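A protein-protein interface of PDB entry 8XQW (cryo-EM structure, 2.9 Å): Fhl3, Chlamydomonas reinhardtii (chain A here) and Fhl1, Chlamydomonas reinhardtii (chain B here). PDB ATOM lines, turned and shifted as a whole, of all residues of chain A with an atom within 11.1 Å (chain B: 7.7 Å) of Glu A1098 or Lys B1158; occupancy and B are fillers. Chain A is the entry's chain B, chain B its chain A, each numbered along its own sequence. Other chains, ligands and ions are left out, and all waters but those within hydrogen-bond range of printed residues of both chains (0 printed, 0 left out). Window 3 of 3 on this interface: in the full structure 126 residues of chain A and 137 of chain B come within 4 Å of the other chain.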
ATOM      1  N   THR A 950      -2.483   2.032  -4.537  1.00  0.00           N
ATOM      2  CA  THR A 950      -1.754   0.836  -4.139  1.00  0.00           C
ATOM      3  C   THR A 950      -2.310  -0.405  -4.820  1.00  0.00           C
ATOM      4  O   THR A 950      -1.547  -1.291  -5.208  1.00  0.00           O
ATOM      5  CB  THR A 950      -1.799   0.694  -2.627  1.00  0.00           C
ATOM      6  OG1 THR A 950      -1.273   1.885  -2.040  1.00  0.00           O
ATOM      7  CG2 THR A 950      -0.969  -0.467  -2.182  1.00  0.00           C
ATOM      8  N   GLU A 951      -3.628  -0.482  -4.992  1.00  0.00           N
ATOM      9  CA  GLU A 951      -4.213  -1.633  -5.671  1.00  0.00           C
ATOM     10  C   GLU A 951      -3.689  -1.762  -7.091  1.00  0.00           C
ATOM     11  O   GLU A 951      -3.157  -2.808  -7.483  1.00  0.00           O
ATOM     12  CB  GLU A 951      -5.731  -1.514  -5.678  1.00  0.00           C
ATOM     13  CG  GLU A 951      -6.368  -1.719  -4.327  1.00  0.00           C
ATOM     14  CD  GLU A 951      -7.713  -2.421  -4.419  1.00  0.00           C
ATOM     15  OE1 GLU A 951      -8.264  -2.502  -5.535  1.00  0.00           O
ATOM     16  OE2 GLU A 951      -8.223  -2.889  -3.379  1.00  0.00           O
ATOM     17  N   ARG A 954       0.095  -2.541  -7.277  1.00  0.00           N
ATOM     18  CA  ARG A 954       0.448  -3.915  -6.944  1.00  0.00           C
ATOM     19  C   ARG A 954       0.051  -4.870  -8.055  1.00  0.00           C
ATOM     20  O   ARG A 954       0.797  -5.802  -8.381  1.00  0.00           O
ATOM     21  CB  ARG A 954      -0.208  -4.322  -5.635  1.00  0.00           C
ATOM     22  CG  ARG A 954       0.361  -3.641  -4.432  1.00  0.00           C
ATOM     23  CD  ARG A 954       1.852  -3.616  -4.475  1.00  0.00           C
ATOM     24  NE  ARG A 954       2.401  -3.104  -3.231  1.00  0.00           N
ATOM     25  CZ  ARG A 954       3.267  -2.105  -3.155  1.00  0.00           C
ATOM     26  NH1 ARG A 954       3.695  -1.515  -4.252  1.00  0.00           N
ATOM     27  NH2 ARG A 954       3.714  -1.704  -1.980  1.00  0.00           N
ATOM     28  N   SER A1094      -7.706 -11.146  -7.353  1.00  0.00           N
ATOM     29  CA  SER A1094      -8.182 -10.334  -6.245  1.00  0.00           C
ATOM     30  C   SER A1094      -6.989  -9.755  -5.508  1.00  0.00           C
ATOM     31  O   SER A1094      -5.880 -10.281  -5.577  1.00  0.00           O
ATOM     32  CB  SER A1094      -9.048 -11.150  -5.296  1.00  0.00           C
ATOM     33  OG  SER A1094      -8.578 -12.480  -5.235  1.00  0.00           O
ATOM     34  N   VAL A1095      -7.231  -8.654  -4.810  1.00  0.00           N
ATOM     35  CA  VAL A1095      -6.215  -7.974  -4.021  1.00  0.00           C
ATOM     36  C   VAL A1095      -6.737  -7.857  -2.601  1.00  0.00           C
ATOM     37  O   VAL A1095      -7.885  -7.452  -2.395  1.00  0.00           O
ATOM     38  CB  VAL A1095      -5.887  -6.583  -4.587  1.00  0.00           C
ATOM     39  CG1 VAL A1095      -4.589  -6.070  -4.006  1.00  0.00           C
ATOM     40  CG2 VAL A1095      -5.810  -6.637  -6.083  1.00  0.00           C
ATOM     41  N   LYS A1096      -5.911  -8.211  -1.625  1.00  0.00           N
ATOM     42  CA  LYS A1096      -6.335  -8.211  -0.232  1.00  0.00           C
ATOM     43  C   LYS A1096      -5.776  -6.989   0.485  1.00  0.00           C
ATOM     44  O   LYS A1096      -4.569  -6.739   0.452  1.00  0.00           O
ATOM     45  CB  LYS A1096      -5.913  -9.496   0.473  1.00  0.00           C
ATOM     46  CG  LYS A1096      -4.435  -9.767   0.499  1.00  0.00           C
ATOM     47  CD  LYS A1096      -4.063 -10.480   1.782  1.00  0.00           C
ATOM     48  CE  LYS A1096      -2.626 -10.956   1.762  1.00  0.00           C
ATOM     49  NZ  LYS A1096      -2.482 -12.244   1.031  1.00  0.00           N
ATOM     50  N   THR A1097      -6.659  -6.228   1.124  1.00  0.00           N
ATOM     51  CA  THR A1097      -6.283  -5.075   1.924  1.00  0.00           C
ATOM     52  C   THR A1097      -7.112  -5.070   3.199  1.00  0.00           C
ATOM     53  O   THR A1097      -8.247  -5.544   3.222  1.00  0.00           O
ATOM     54  CB  THR A1097      -6.496  -3.766   1.167  1.00  0.00           C
ATOM     55  OG1 THR A1097      -7.807  -3.760   0.596  1.00  0.00           O
ATOM     56  CG2 THR A1097      -5.478  -3.614   0.061  1.00  0.00           C
ATOM     57  N   GLU A1098      -6.534  -4.521   4.264  1.00  0.00           N
ATOM     58  CA  GLU A1098      -7.183  -4.497   5.576  1.00  0.00           C
ATOM     59  C   GLU A1098      -7.205  -3.061   6.086  1.00  0.00           C
ATOM     60  O   GLU A1098      -6.224  -2.591   6.662  1.00  0.00           O
ATOM     61  CB  GLU A1098      -6.460  -5.406   6.557  1.00  0.00           C
ATOM     62  CG  GLU A1098      -6.399  -6.849   6.135  1.00  0.00           C
ATOM     63  CD  GLU A1098      -5.191  -7.144   5.284  1.00  0.00           C
ATOM     64  OE1 GLU A1098      -4.703  -6.216   4.610  1.00  0.00           O
ATOM     65  OE2 GLU A1098      -4.721  -8.299   5.292  1.00  0.00           O
ATOM     66  N   LEU A1099      -8.268  -2.418   5.907  1.00  0.00           N
ATOM     67  CA  LEU A1099      -8.234  -1.042   6.351  1.00  0.00           C
ATOM     68  C   LEU A1099      -8.769  -0.910   7.769  1.00  0.00           C
ATOM     69  O   LEU A1099      -9.661  -1.656   8.173  1.00  0.00           O
ATOM     70  CB  LEU A1099      -9.065  -0.170   5.417  1.00  0.00           C
ATOM     71  CG  LEU A1099      -8.678  -0.343   3.960  1.00  0.00           C
ATOM     72  CD1 LEU A1099      -9.551   0.520   3.096  1.00  0.00           C
ATOM     73  CD2 LEU A1099      -7.236   0.016   3.775  1.00  0.00           C
ATOM     74  N   PRO A1100      -8.251   0.031   8.549  1.00  0.00           N
ATOM     75  CA  PRO A1100      -8.788   0.259   9.891  1.00  0.00           C
ATOM     76  C   PRO A1100     -10.203   0.803   9.822  1.00  0.00           C
ATOM     77  O   PRO A1100     -10.815   0.890   8.761  1.00  0.00           O
ATOM     78  CB  PRO A1100      -7.824   1.284  10.482  1.00  0.00           C
ATOM     79  CG  PRO A1100      -6.602   1.130   9.699  1.00  0.00           C
ATOM     80  CD  PRO A1100      -7.031   0.810   8.325  1.00  0.00           C
ATOM     81  N   ASP A1101     -10.739   1.161  10.986  1.00  0.00           N
ATOM     82  CA  ASP A1101     -12.112   1.645  11.007  1.00  0.00           C
ATOM     83  C   ASP A1101     -12.204   3.155  10.850  1.00  0.00           C
ATOM     84  O   ASP A1101     -13.149   3.648  10.223  1.00  0.00           O
ATOM     85  CB  ASP A1101     -12.802   1.207  12.290  1.00  0.00           C
ATOM     86  CG  ASP A1101     -13.699   0.012  12.077  1.00  0.00           C
ATOM     87  OD1 ASP A1101     -14.611   0.096  11.229  1.00  0.00           O
ATOM     88  OD2 ASP A1101     -13.495  -1.016  12.752  1.00  0.00           O
ATOM     89  N   TRP A1102     -11.256   3.903  11.406  1.00  0.00           N
ATOM     90  CA  TRP A1102     -11.250   5.339  11.175  1.00  0.00           C
ATOM     91  C   TRP A1102     -11.097   5.641   9.695  1.00  0.00           C
ATOM     92  O   TRP A1102     -11.685   6.602   9.182  1.00  0.00           O
ATOM     93  CB  TRP A1102     -10.139   5.999  11.985  1.00  0.00           C
ATOM     94  CG  TRP A1102      -8.786   5.481  11.692  1.00  0.00           C
ATOM     95  CD1 TRP A1102      -8.160   4.449  12.302  1.00  0.00           C
ATOM     96  CD2 TRP A1102      -7.876   5.982  10.718  1.00  0.00           C
ATOM     97  NE1 TRP A1102      -6.917   4.264  11.765  1.00  0.00           N
ATOM     98  CE2 TRP A1102      -6.721   5.197  10.785  1.00  0.00           C
ATOM     99  CE3 TRP A1102      -7.932   7.013   9.784  1.00  0.00           C
ATOM    100  CZ2 TRP A1102      -5.637   5.411   9.960  1.00  0.00           C
ATOM    101  CZ3 TRP A1102      -6.857   7.221   8.972  1.00  0.00           C
ATOM    102  CH2 TRP A1102      -5.724   6.428   9.064  1.00  0.00           C
ATOM    103  N   TYR A1103     -10.348   4.805   8.982  1.00  0.00           N
ATOM    104  CA  TYR A1103     -10.193   5.001   7.549  1.00  0.00           C
ATOM    105  C   TYR A1103     -11.502   4.777   6.817  1.00  0.00           C
ATOM    106  O   TYR A1103     -11.823   5.502   5.873  1.00  0.00           O
ATOM    107  CB  TYR A1103      -9.126   4.072   7.002  1.00  0.00           C
ATOM    108  CG  TYR A1103      -8.685   4.461   5.631  1.00  0.00           C
ATOM    109  CD1 TYR A1103      -7.871   5.555   5.439  1.00  0.00           C
ATOM    110  CD2 TYR A1103      -9.096   3.752   4.528  1.00  0.00           C
ATOM    111  CE1 TYR A1103      -7.470   5.923   4.195  1.00  0.00           C
ATOM    112  CE2 TYR A1103      -8.705   4.114   3.277  1.00  0.00           C
ATOM    113  CZ  TYR A1103      -7.889   5.201   3.113  1.00  0.00           C
ATOM    114  OH  TYR A1103      -7.489   5.572   1.856  1.00  0.00           O
ATOM    115  N   LYS A1104     -12.275   3.780   7.230  1.00  0.00           N
ATOM    116  CA  LYS A1104     -13.550   3.546   6.576  1.00  0.00           C
ATOM    117  C   LYS A1104     -14.531   4.666   6.869  1.00  0.00           C
ATOM    118  O   LYS A1104     -15.309   5.058   5.994  1.00  0.00           O
ATOM    119  CB  LYS A1104     -14.107   2.199   7.002  1.00  0.00           C
ATOM    120  CG  LYS A1104     -13.396   1.055   6.338  1.00  0.00           C
ATOM    121  CD  LYS A1104     -13.777  -0.264   6.947  1.00  0.00           C
ATOM    122  CE  LYS A1104     -13.202  -1.406   6.145  1.00  0.00           C
ATOM    123  NZ  LYS A1104     -13.112  -2.648   6.953  1.00  0.00           N
ATOM    124  N   VAL A1107     -13.481   7.419   4.411  1.00  0.00           N
ATOM    125  CA  VAL A1107     -13.844   7.225   3.008  1.00  0.00           C
ATOM    126  C   VAL A1107     -15.349   7.198   2.832  1.00  0.00           C
ATOM    127  O   VAL A1107     -15.844   7.405   1.722  1.00  0.00           O
ATOM    128  CB  VAL A1107     -13.217   5.958   2.406  1.00  0.00           C
ATOM    129  CG1 VAL A1107     -11.781   5.833   2.810  1.00  0.00           C
ATOM    130  CG2 VAL A1107     -14.006   4.740   2.795  1.00  0.00           C
ATOM    131  N   SER B1129      -0.981  -9.388  -2.635  1.00  0.00           N
ATOM    132  CA  SER B1129      -0.952  -8.805  -1.306  1.00  0.00           C
ATOM    133  C   SER B1129      -0.644  -7.320  -1.370  1.00  0.00           C
ATOM    134  O   SER B1129      -0.005  -6.834  -2.300  1.00  0.00           O
ATOM    135  CB  SER B1129       0.089  -9.501  -0.448  1.00  0.00           C
ATOM    136  OG  SER B1129       1.319  -9.534  -1.135  1.00  0.00           O
ATOM    137  N   TRP B1130      -1.089  -6.602  -0.346  1.00  0.00           N
ATOM    138  CA  TRP B1130      -0.883  -5.165  -0.299  1.00  0.00           C
ATOM    139  C   TRP B1130       0.575  -4.779  -0.146  1.00  0.00           C
ATOM    140  O   TRP B1130       0.897  -3.598  -0.291  1.00  0.00           O
ATOM    141  CB  TRP B1130      -1.683  -4.569   0.849  1.00  0.00           C
ATOM    142  CG  TRP B1130      -1.249  -5.061   2.182  1.00  0.00           C
ATOM    143  CD1 TRP B1130      -1.672  -6.186   2.810  1.00  0.00           C
ATOM    144  CD2 TRP B1130      -0.315  -4.439   3.060  1.00  0.00           C
ATOM    145  NE1 TRP B1130      -1.052  -6.313   4.021  1.00  0.00           N
ATOM    146  CE2 TRP B1130      -0.213  -5.248   4.198  1.00  0.00           C
ATOM    147  CE3 TRP B1130       0.455  -3.280   2.991  1.00  0.00           C
ATOM    148  CZ2 TRP B1130       0.621  -4.935   5.253  1.00  0.00           C
ATOM    149  CZ3 TRP B1130       1.275  -2.973   4.039  1.00  0.00           C
ATOM    150  CH2 TRP B1130       1.357  -3.795   5.152  1.00  0.00           C
ATOM    151  N   SER B1131       1.456  -5.726   0.137  1.00  0.00           N
ATOM    152  CA  SER B1131       2.854  -5.434   0.404  1.00  0.00           C
ATOM    153  C   SER B1131       3.728  -5.919  -0.738  1.00  0.00           C
ATOM    154  O   SER B1131       3.500  -6.994  -1.290  1.00  0.00           O
ATOM    155  CB  SER B1131       3.307  -6.097   1.693  1.00  0.00           C
ATOM    156  OG  SER B1131       4.693  -6.329   1.646  1.00  0.00           O
ATOM    157  N   GLU B1134       5.876  -9.289  -0.051  1.00  0.00           N
ATOM    158  CA  GLU B1134       5.279 -10.601  -0.233  1.00  0.00           C
ATOM    159  C   GLU B1134       5.187 -11.002  -1.691  1.00  0.00           C
ATOM    160  O   GLU B1134       4.912 -12.167  -1.979  1.00  0.00           O
ATOM    161  CB  GLU B1134       3.891 -10.627   0.382  1.00  0.00           C
ATOM    162  CG  GLU B1134       3.872 -10.666   1.881  1.00  0.00           C
ATOM    163  CD  GLU B1134       2.500 -11.014   2.411  1.00  0.00           C
ATOM    164  OE1 GLU B1134       1.608 -10.142   2.368  1.00  0.00           O
ATOM    165  OE2 GLU B1134       2.304 -12.163   2.852  1.00  0.00           O
ATOM    166  N   VAL B1142      10.661 -14.032   3.699  1.00  0.00           N
ATOM    167  CA  VAL B1142       9.871 -13.000   4.361  1.00  0.00           C
ATOM    168  C   VAL B1142       9.901 -13.199   5.865  1.00  0.00           C
ATOM    169  O   VAL B1142      10.158 -12.262   6.625  1.00  0.00           O
ATOM    170  CB  VAL B1142       8.433 -12.993   3.827  1.00  0.00           C
ATOM    171  CG1 VAL B1142       7.538 -12.292   4.796  1.00  0.00           C
ATOM    172  CG2 VAL B1142       8.383 -12.308   2.500  1.00  0.00           C
ATOM    173  N   LYS B1146      11.457  -9.842   7.580  1.00  0.00           N
ATOM    174  CA  LYS B1146      10.445  -8.822   7.799  1.00  0.00           C
ATOM    175  C   LYS B1146      10.709  -7.959   9.016  1.00  0.00           C
ATOM    176  O   LYS B1146      10.037  -6.939   9.177  1.00  0.00           O
ATOM    177  CB  LYS B1146       9.077  -9.467   7.936  1.00  0.00           C
ATOM    178  CG  LYS B1146       8.849 -10.109   9.266  1.00  0.00           C
ATOM    179  CD  LYS B1146       7.498 -10.748   9.310  1.00  0.00           C
ATOM    180  CE  LYS B1146       7.190 -11.246  10.685  1.00  0.00           C
ATOM    181  NZ  LYS B1146       5.823 -11.805  10.728  1.00  0.00           N
ATOM    182  N   THR B1152       5.197   0.074  10.992  1.00  0.00           N
ATOM    183  CA  THR B1152       4.760  -0.072  12.365  1.00  0.00           C
ATOM    184  C   THR B1152       4.642  -1.547  12.716  1.00  0.00           C
ATOM    185  O   THR B1152       4.643  -2.416  11.848  1.00  0.00           O
ATOM    186  CB  THR B1152       3.419   0.613  12.571  1.00  0.00           C
ATOM    187  OG1 THR B1152       2.375  -0.345  12.409  1.00  0.00           O
ATOM    188  CG2 THR B1152       3.228   1.675  11.532  1.00  0.00           C
ATOM    189  N   GLU B1153       4.533  -1.832  14.010  1.00  0.00           N
ATOM    190  CA  GLU B1153       4.452  -3.222  14.433  1.00  0.00           C
ATOM    191  C   GLU B1153       3.168  -3.896  13.984  1.00  0.00           C
ATOM    192  O   GLU B1153       3.191  -5.084  13.647  1.00  0.00           O
ATOM    193  CB  GLU B1153       4.578  -3.320  15.946  1.00  0.00           C
ATOM    194  CG  GLU B1153       5.981  -3.083  16.431  1.00  0.00           C
ATOM    195  CD  GLU B1153       6.964  -4.042  15.803  1.00  0.00           C
ATOM    196  OE1 GLU B1153       8.056  -3.596  15.399  1.00  0.00           O
ATOM    197  OE2 GLU B1153       6.643  -5.244  15.709  1.00  0.00           O
ATOM    198  N   GLY B1154       2.053  -3.171  13.966  1.00  0.00           N
ATOM    199  CA  GLY B1154       0.814  -3.762  13.502  1.00  0.00           C
ATOM    200  C   GLY B1154       0.856  -4.145  12.043  1.00  0.00           C
ATOM    201  O   GLY B1154       0.106  -5.019  11.608  1.00  0.00           O
ATOM    202  N   ALA B1155       1.721  -3.498  11.264  1.00  0.00           N
ATOM    203  CA  ALA B1155       1.888  -3.883   9.872  1.00  0.00           C
ATOM    204  C   ALA B1155       2.767  -5.112   9.745  1.00  0.00           C
ATOM    205  O   ALA B1155       2.411  -6.061   9.047  1.00  0.00           O
ATOM    206  CB  ALA B1155       2.485  -2.732   9.074  1.00  0.00           C
ATOM    207  N   ILE B1156       3.914  -5.111  10.422  1.00  0.00           N
ATOM    208  CA  ILE B1156       4.818  -6.252  10.369  1.00  0.00           C
ATOM    209  C   ILE B1156       4.126  -7.511  10.859  1.00  0.00           C
ATOM    210  O   ILE B1156       4.382  -8.606  10.352  1.00  0.00           O
ATOM    211  CB  ILE B1156       6.084  -5.942  11.181  1.00  0.00           C
ATOM    212  CG1 ILE B1156       7.079  -5.169  10.331  1.00  0.00           C
ATOM    213  CG2 ILE B1156       6.717  -7.199  11.701  1.00  0.00           C
ATOM    214  CD1 ILE B1156       8.180  -4.561  11.137  1.00  0.00           C
ATOM    215  N   ALA B1157       3.221  -7.386  11.820  1.00  0.00           N
ATOM    216  CA  ALA B1157       2.535  -8.575  12.304  1.00  0.00           C
ATOM    217  C   ALA B1157       1.558  -9.161  11.297  1.00  0.00           C
ATOM    218  O   ALA B1157       0.939 -10.181  11.599  1.00  0.00           O
ATOM    219  CB  ALA B1157       1.798  -8.261  13.599  1.00  0.00           C
ATOM    220  N   LYS B1158       1.400  -8.562  10.119  1.00  0.00           N
ATOM    221  CA  LYS B1158       0.459  -9.044   9.119  1.00  0.00           C
ATOM    222  C   LYS B1158       1.140  -9.755   7.959  1.00  0.00           C
ATOM    223  O   LYS B1158       0.481 -10.060   6.965  1.00  0.00           O
ATOM    224  CB  LYS B1158      -0.377  -7.885   8.578  1.00  0.00           C
ATOM    225  CG  LYS B1158      -1.536  -7.498   9.448  1.00  0.00           C
ATOM    226  CD  LYS B1158      -2.297  -6.335   8.850  1.00  0.00           C
ATOM    227  CE  LYS B1158      -3.419  -5.901   9.767  1.00  0.00           C
ATOM    228  NZ  LYS B1158      -4.155  -4.725   9.243  1.00  0.00           N
ATOM    229  N   LEU B1159       2.435 -10.021   8.053  1.00  0.00           N
ATOM    230  CA  LEU B1159       3.192 -10.586   6.949  1.00  0.00           C
ATOM    231  C   LEU B1159       3.784 -11.924   7.358  1.00  0.00           C
ATOM    232  O   LEU B1159       4.256 -12.082   8.485  1.00  0.00           O
ATOM    233  CB  LEU B1159       4.306  -9.642   6.517  1.00  0.00           C
ATOM    234  CG  LEU B1159       3.904  -8.182   6.370  1.00  0.00           C
ATOM    235  CD1 LEU B1159       5.077  -7.358   5.933  1.00  0.00           C
ATOM    236  CD2 LEU B1159       2.792  -8.069   5.372  1.00  0.00           C
ATOM    237  N   GLY B1160       3.767 -12.879   6.435  1.00  0.00           N
ATOM    238  CA  GLY B1160       4.336 -14.180   6.685  1.00  0.00           C
ATOM    239  C   GLY B1160       3.313 -15.184   7.174  1.00  0.00           C
ATOM    240  O   GLY B1160       2.155 -15.181   6.751  1.00  0.00           O
ATOM    241  N   PRO B1161       3.724 -16.062   8.083  1.00  0.00           N
ATOM    242  CA  PRO B1161       2.819 -17.090   8.580  1.00  0.00           C
ATOM    243  C   PRO B1161       1.761 -16.473   9.470  1.00  0.00           C
ATOM    244  O   PRO B1161       2.079 -15.734  10.412  1.00  0.00           O
ATOM    245  CB  PRO B1161       3.741 -18.025   9.381  1.00  0.00           C
ATOM    246  CG  PRO B1161       5.132 -17.522   9.152  1.00  0.00           C
ATOM    247  CD  PRO B1161       5.001 -16.086   8.801  1.00  0.00           C
ATOM    248  N   PRO B1162       0.486 -16.772   9.218  1.00  0.00           N
ATOM    249  CA  PRO B1162      -0.587 -16.094   9.959  1.00  0.00           C
ATOM    250  C   PRO B1162      -0.570 -16.364  11.449  1.00  0.00           C
ATOM    251  O   PRO B1162      -1.445 -15.847  12.155  1.00  0.00           O
ATOM    252  CB  PRO B1162      -1.864 -16.649   9.313  1.00  0.00           C
ATOM    253  CG  PRO B1162      -1.422 -17.186   7.985  1.00  0.00           C
ATOM    254  CD  PRO B1162      -0.037 -17.692   8.199  1.00  0.00           C
ATOM    255  N   ALA B1164       1.391 -15.250  13.786  1.00  0.00           N
ATOM    256  CA  ALA B1164       1.610 -13.992  14.490  1.00  0.00           C
ATOM    257  C   ALA B1164       1.907 -14.222  15.968  1.00  0.00           C
ATOM    258  O   ALA B1164       2.541 -15.209  16.333  1.00  0.00           O
ATOM    259  CB  ALA B1164       0.408 -13.073  14.327  1.00  0.00           C
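The guanidinium group (NE) of Arg A954 sits at hydrogen-bond distance from the backbone carbonyl oxygen (O) of Trp B1130 (3.3 Å).
The side-chain hydroxyl of Ser B1129 is in hydrogen-bond range of the backbone carbonyl oxygen of Ser B1131 (3.4 Å).
CG of Arg A954 touches O of Ser B1129, 3.9 Å away.
Arg A954 touches Ser B1131.
Lys A1096 touches Ser B1129.
Lys A1096 touches Trp B1130 (O to N, 3.6 Å).
Trp B1130 touches Thr A1097.
Glu A1098 touches Trp B1130.
Glu A1098 touches Lys B1158 (CB to NZ, 3.6 Å).
Of the printed residues of chain B, Arg A954 touches Ser B1129, Trp B1130 and Ser B1131.
Of chain B, only Trp B1130 and Lys B1158 come within 4 Å of Glu A1098.
Printed residues of chain A within 4 Å of Ser B1131: Arg A954.
Glu B1153 touches none of the printed residues of chain A.
No residue of chain A comes within 4 Å of Gly B1154.
No residue of chain A comes within 4 Å of Ala B1155.
Lys B1158 touches one residue of chain A.
The nearest residue of chain A that does not touch Lys B1158 is Leu A1099 (5.8 Å).
The nearest printed residue of chain A that does not touch Ser B1129 is Val A1095 (4.9 Å).
Of the 15 printed residues of chain A, 4 touch a printed residue of chain B.
Hydrophobic or aromatic side chains of chain B that line the printed part of chain A: Trp B1130.
Among the printed residues, 8 pairs touch across the chains.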
